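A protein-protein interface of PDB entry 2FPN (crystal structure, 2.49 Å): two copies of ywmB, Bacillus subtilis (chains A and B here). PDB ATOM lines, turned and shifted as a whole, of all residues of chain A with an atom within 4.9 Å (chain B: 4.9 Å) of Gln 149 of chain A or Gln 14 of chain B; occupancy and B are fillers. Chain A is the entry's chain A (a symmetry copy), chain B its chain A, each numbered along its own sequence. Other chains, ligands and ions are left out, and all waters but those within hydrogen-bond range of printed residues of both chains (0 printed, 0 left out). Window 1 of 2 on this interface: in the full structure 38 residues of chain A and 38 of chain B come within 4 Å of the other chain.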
ATOM      1  N   LYS A 145       2.050  -0.858   2.073  1.00  0.00           N
ATOM      2  CA  LYS A 145       1.515  -2.036   2.747  1.00  0.00           C
ATOM      3  C   LYS A 145       1.999  -2.095   4.198  1.00  0.00           C
ATOM      4  O   LYS A 145       1.189  -2.236   5.126  1.00  0.00           O
ATOM      5  CB  LYS A 145       1.851  -3.318   1.962  1.00  0.00           C
ATOM      6  CG  LYS A 145       1.509  -4.648   2.667  1.00  0.00           C
ATOM      7  CD  LYS A 145       0.060  -4.712   3.180  1.00  0.00           C
ATOM      8  CE  LYS A 145      -0.198  -6.007   3.945  1.00  0.00           C
ATOM      9  NZ  LYS A 145      -1.328  -5.858   4.895  1.00  0.00           N
ATOM     10  N   LYS A 146       3.314  -1.961   4.378  1.00  0.00           N
ATOM     11  CA  LYS A 146       3.935  -1.959   5.706  1.00  0.00           C
ATOM     12  C   LYS A 146       3.403  -0.826   6.581  1.00  0.00           C
ATOM     13  O   LYS A 146       3.149  -1.022   7.773  1.00  0.00           O
ATOM     14  CB  LYS A 146       5.465  -1.893   5.596  1.00  0.00           C
ATOM     15  CG  LYS A 146       6.217  -2.109   6.914  1.00  0.00           C
ATOM     16  CD  LYS A 146       6.006  -3.504   7.490  1.00  0.00           C
ATOM     17  CE  LYS A 146       6.956  -4.516   6.886  1.00  0.00           C
ATOM     18  NZ  LYS A 146       6.825  -5.833   7.559  1.00  0.00           N
ATOM     19  N   ALA A 147       3.223   0.346   5.974  1.00  0.00           N
ATOM     20  CA  ALA A 147       2.602   1.490   6.638  1.00  0.00           C
ATOM     21  C   ALA A 147       1.297   1.086   7.317  1.00  0.00           C
ATOM     22  O   ALA A 147       1.081   1.401   8.485  1.00  0.00           O
ATOM     23  CB  ALA A 147       2.368   2.616   5.643  1.00  0.00           C
ATOM     24  N   ASN A 148       0.448   0.369   6.584  1.00  0.00           N
ATOM     25  CA  ASN A 148      -0.833  -0.113   7.100  1.00  0.00           C
ATOM     26  C   ASN A 148      -0.668  -1.172   8.174  1.00  0.00           C
ATOM     27  O   ASN A 148      -1.295  -1.100   9.232  1.00  0.00           O
ATOM     28  CB  ASN A 148      -1.703  -0.647   5.962  1.00  0.00           C
ATOM     29  CG  ASN A 148      -2.330   0.465   5.144  1.00  0.00           C
ATOM     30  OD1 ASN A 148      -2.011   0.638   3.964  1.00  0.00           O
ATOM     31  ND2 ASN A 148      -3.218   1.239   5.775  1.00  0.00           N
ATOM     32  N   GLN A 149       0.182  -2.153   7.893  1.00  0.00           N
ATOM     33  CA  GLN A 149       0.510  -3.177   8.868  1.00  0.00           C
ATOM     34  C   GLN A 149       0.877  -2.503  10.183  1.00  0.00           C
ATOM     35  O   GLN A 149       0.382  -2.897  11.238  1.00  0.00           O
ATOM     36  CB  GLN A 149       1.660  -4.040   8.361  1.00  0.00           C
ATOM     37  CG  GLN A 149       1.329  -4.885   7.143  1.00  0.00           C
ATOM     38  CD  GLN A 149       2.549  -5.608   6.587  1.00  0.00           C
ATOM     39  OE1 GLN A 149       3.377  -5.022   5.895  1.00  0.00           O
ATOM     40  NE2 GLN A 149       2.658  -6.891   6.892  1.00  0.00           N
ATOM     41  N   LEU A 150       1.716  -1.467  10.095  1.00  0.00           N
ATOM     42  CA  LEU A 150       2.112  -0.644  11.247  1.00  0.00           C
ATOM     43  C   LEU A 150       0.941   0.125  11.847  1.00  0.00           C
ATOM     44  O   LEU A 150       0.780   0.162  13.067  1.00  0.00           O
ATOM     45  CB  LEU A 150       3.228   0.346  10.869  1.00  0.00           C
ATOM     46  CG  LEU A 150       4.684  -0.123  10.771  1.00  0.00           C
ATOM     47  CD1 LEU A 150       5.533   0.908  10.040  1.00  0.00           C
ATOM     48  CD2 LEU A 150       5.275  -0.440  12.140  1.00  0.00           C
ATOM     49  N   LEU A 151       0.135   0.740  10.984  1.00  0.00           N
ATOM     50  CA  LEU A 151      -1.043   1.494  11.411  1.00  0.00           C
ATOM     51  C   LEU A 151      -1.988   0.612  12.222  1.00  0.00           C
ATOM     52  O   LEU A 151      -2.535   1.046  13.235  1.00  0.00           O
ATOM     53  CB  LEU A 151      -1.767   2.099  10.200  1.00  0.00           C
ATOM     54  CG  LEU A 151      -3.044   2.926  10.400  1.00  0.00           C
ATOM     55  CD1 LEU A 151      -2.798   4.110  11.318  1.00  0.00           C
ATOM     56  CD2 LEU A 151      -3.597   3.391   9.058  1.00  0.00           C
ATOM     57  N   ASN A 152      -2.160  -0.628  11.767  1.00  0.00           N
ATOM     58  CA  ASN A 152      -2.991  -1.600  12.463  1.00  0.00           C
ATOM     59  C   ASN A 152      -2.268  -2.202  13.656  1.00  0.00           C
ATOM     60  O   ASN A 152      -2.881  -2.447  14.699  1.00  0.00           O
ATOM     61  CB  ASN A 152      -3.471  -2.681  11.501  1.00  0.00           C
ATOM     62  CG  ASN A 152      -4.319  -2.117  10.370  1.00  0.00           C
ATOM     63  OD1 ASN A 152      -4.200  -2.542   9.220  1.00  0.00           O
ATOM     64  ND2 ASN A 152      -5.173  -1.148  10.690  1.00  0.00           N
ATOM     65  N   GLU A 153      -0.975  -2.440  13.485  1.00  0.00           N
ATOM     66  CA  GLU A 153      -0.115  -2.771  14.602  1.00  0.00           C
ATOM     67  C   GLU A 153      -0.460  -1.897  15.784  1.00  0.00           C
ATOM     68  O   GLU A 153      -0.310  -2.302  16.930  1.00  0.00           O
ATOM     69  CB  GLU A 153       1.347  -2.584  14.222  1.00  0.00           C
ATOM     70  CG  GLU A 153       2.319  -3.268  15.164  1.00  0.00           C
ATOM     71  CD  GLU A 153       2.069  -4.754  15.293  1.00  0.00           C
ATOM     72  OE1 GLU A 153       2.137  -5.455  14.269  1.00  0.00           O
ATOM     73  OE2 GLU A 153       1.810  -5.224  16.418  1.00  0.00           O
ATOM     74  N   GLY B  10       6.131  -2.752  18.810  1.00  0.00           N
ATOM     75  CA  GLY B  10       5.299  -2.749  17.618  1.00  0.00           C
ATOM     76  C   GLY B  10       6.135  -2.773  16.362  1.00  0.00           C
ATOM     77  O   GLY B  10       5.792  -3.459  15.402  1.00  0.00           O
ATOM     78  N   MET B  11       7.248  -2.044  16.362  1.00  0.00           N
ATOM     79  CA  MET B  11       8.108  -1.981  15.176  1.00  0.00           C
ATOM     80  C   MET B  11       8.851  -3.295  14.875  1.00  0.00           C
ATOM     81  O   MET B  11       8.938  -3.702  13.712  1.00  0.00           O
ATOM     82  CB  MET B  11       9.081  -0.808  15.255  1.00  0.00           C
ATOM     83  CG  MET B  11       8.461   0.516  14.839  1.00  0.00           C
ATOM     84  SD  MET B  11       9.468   1.909  15.363  1.00  0.00           S
ATOM     85  CE  MET B  11      10.656   1.985  14.021  1.00  0.00           C
ATOM     86  N   GLU B  12       9.375  -3.938  15.922  1.00  0.00           N
ATOM     87  CA  GLU B  12      10.018  -5.245  15.800  1.00  0.00           C
ATOM     88  C   GLU B  12       9.070  -6.275  15.199  1.00  0.00           C
ATOM     89  O   GLU B  12       9.397  -6.901  14.184  1.00  0.00           O
ATOM     90  CB  GLU B  12      10.522  -5.752  17.156  1.00  0.00           C
ATOM     91  CG  GLU B  12      11.973  -5.406  17.471  1.00  0.00           C
ATOM     92  CD  GLU B  12      12.126  -4.426  18.632  1.00  0.00           C
ATOM     93  OE1 GLU B  12      11.118  -3.796  19.033  1.00  0.00           O
ATOM     94  OE2 GLU B  12      13.261  -4.283  19.154  1.00  0.00           O
ATOM     95  N   ARG B  13       7.899  -6.434  15.828  1.00  0.00           N
ATOM     96  CA  ARG B  13       6.861  -7.371  15.362  1.00  0.00           C
ATOM     97  C   ARG B  13       6.550  -7.156  13.893  1.00  0.00           C
ATOM     98  O   ARG B  13       6.316  -8.100  13.157  1.00  0.00           O
ATOM     99  CB  ARG B  13       5.576  -7.248  16.191  1.00  0.00           C
ATOM    100  CG  ARG B  13       5.454  -8.307  17.266  1.00  0.00           C
ATOM    101  CD  ARG B  13       4.137  -8.227  18.023  1.00  0.00           C
ATOM    102  NE  ARG B  13       4.280  -7.414  19.224  1.00  0.00           N
ATOM    103  CZ  ARG B  13       3.714  -6.221  19.410  1.00  0.00           C
ATOM    104  NH1 ARG B  13       2.928  -5.693  18.474  1.00  0.00           N
ATOM    105  NH2 ARG B  13       3.930  -5.560  20.544  1.00  0.00           N
ATOM    106  N   GLN B  14       6.575  -5.902  13.473  1.00  0.00           N
ATOM    107  CA  GLN B  14       6.336  -5.558  12.090  1.00  0.00           C
ATOM    108  C   GLN B  14       7.627  -5.603  11.253  1.00  0.00           C
ATOM    109  O   GLN B  14       7.696  -5.034  10.146  1.00  0.00           O
ATOM    110  CB  GLN B  14       5.666  -4.190  12.029  1.00  0.00           C
ATOM    111  CG  GLN B  14       4.751  -3.998  10.857  1.00  0.00           C
ATOM    112  CD  GLN B  14       3.954  -5.241  10.540  1.00  0.00           C
ATOM    113  OE1 GLN B  14       3.168  -5.728  11.362  1.00  0.00           O
ATOM    114  NE2 GLN B  14       4.156  -5.767   9.339  1.00  0.00           N
ATOM    115  N   ASP B  15       8.643  -6.286  11.781  1.00  0.00           N
ATOM    116  CA  ASP B  15       9.906  -6.508  11.064  1.00  0.00           C
ATOM    117  C   ASP B  15      10.715  -5.246  10.757  1.00  0.00           C
ATOM    118  O   ASP B  15      11.544  -5.238   9.843  1.00  0.00           O
ATOM    119  CB  ASP B  15       9.661  -7.284   9.758  1.00  0.00           C
ATOM    120  CG  ASP B  15       9.721  -8.782   9.943  1.00  0.00           C
ATOM    121  OD1 ASP B  15       9.775  -9.472   8.907  1.00  0.00           O
ATOM    122  OD2 ASP B  15       9.715  -9.270  11.098  1.00  0.00           O
ATOM    123  N   VAL B  16      10.470  -4.176  11.504  1.00  0.00           N
ATOM    124  CA  VAL B  16      11.280  -2.972  11.361  1.00  0.00           C
ATOM    125  C   VAL B  16      12.470  -3.045  12.324  1.00  0.00           C
ATOM    126  O   VAL B  16      12.309  -3.298  13.526  1.00  0.00           O
ATOM    127  CB  VAL B  16      10.456  -1.685  11.545  1.00  0.00           C
ATOM    128  CG1 VAL B  16      11.348  -0.447  11.368  1.00  0.00           C
ATOM    129  CG2 VAL B  16       9.283  -1.656  10.556  1.00  0.00           C
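Asp 15 of chain B touches Lys 146 of chain A (CB to NZ, 3.9 Å).
Gln 14 of chain B touches Leu 150 of chain A (CB to CD2, 3.8 Å).
Gly 10 of chain B touches Glu 153 of chain A (O to CG, 3.5 Å).
No position is printed for both chains.
Of the 7 pairs that touch across the chains among the printed residues, none has its exchanged pair printed and touching as well.
N of Lys 146 of chain A lies close to OE1 of Gln 149 of chain A (3.4 Å).
Among the printed residues, 7 pairs touch across the chains.
Among the printed residues, Asp or Glu carboxylates within 4 Å of a Lys or Arg side-chain nitrogen of the other chain: Glu 153 of chain A with Arg 13 of chain B (2.4 Å).
The backbone carbonyl oxygen (O) of Gln 14 of chain B lies within hydrogen-bond range of the side-chain amino group (NZ) of Lys 146 of chain A.
The side-chain amide nitrogen (NE2) of Gln 14 of chain B sits close to the side-chain amide nitrogen (NE2) of Gln 149 of chain A, 3.1 Å away.
OE1 of Glu 153 of chain A lies close to OE1 of Gln 14 of chain B (3.1 Å).
OE2 of Glu 153 of chain A sits close to NH1 of Arg 13 of chain B.
Of the printed residues of chain A, Gln 14 of chain B touches Lys 146 (2.8 Å), Gln 149 (3.1 Å), Leu 150 (3.8 Å) and Glu 153 (3.1 Å).
Of the printed residues of chain A, Gly 10 of chain B touches Glu 153.
Printed residues of chain B within 4 Å of Glu 153 of chain A: Gly 10, Arg 13 and Gln 14.
Of the printed residues of chain B, Leu 150 of chain A touches Gln 14 (3.8 Å).
Of the printed residues of chain B, Lys 146 of chain A touches Gln 14 (2.8 Å) and Asp 15 (3.9 Å).
Of the printed residues of chain A, Arg 13 of chain B touches Glu 153 (2.4 Å).
Leu 151 of chain A touches none of the printed residues of chain B.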
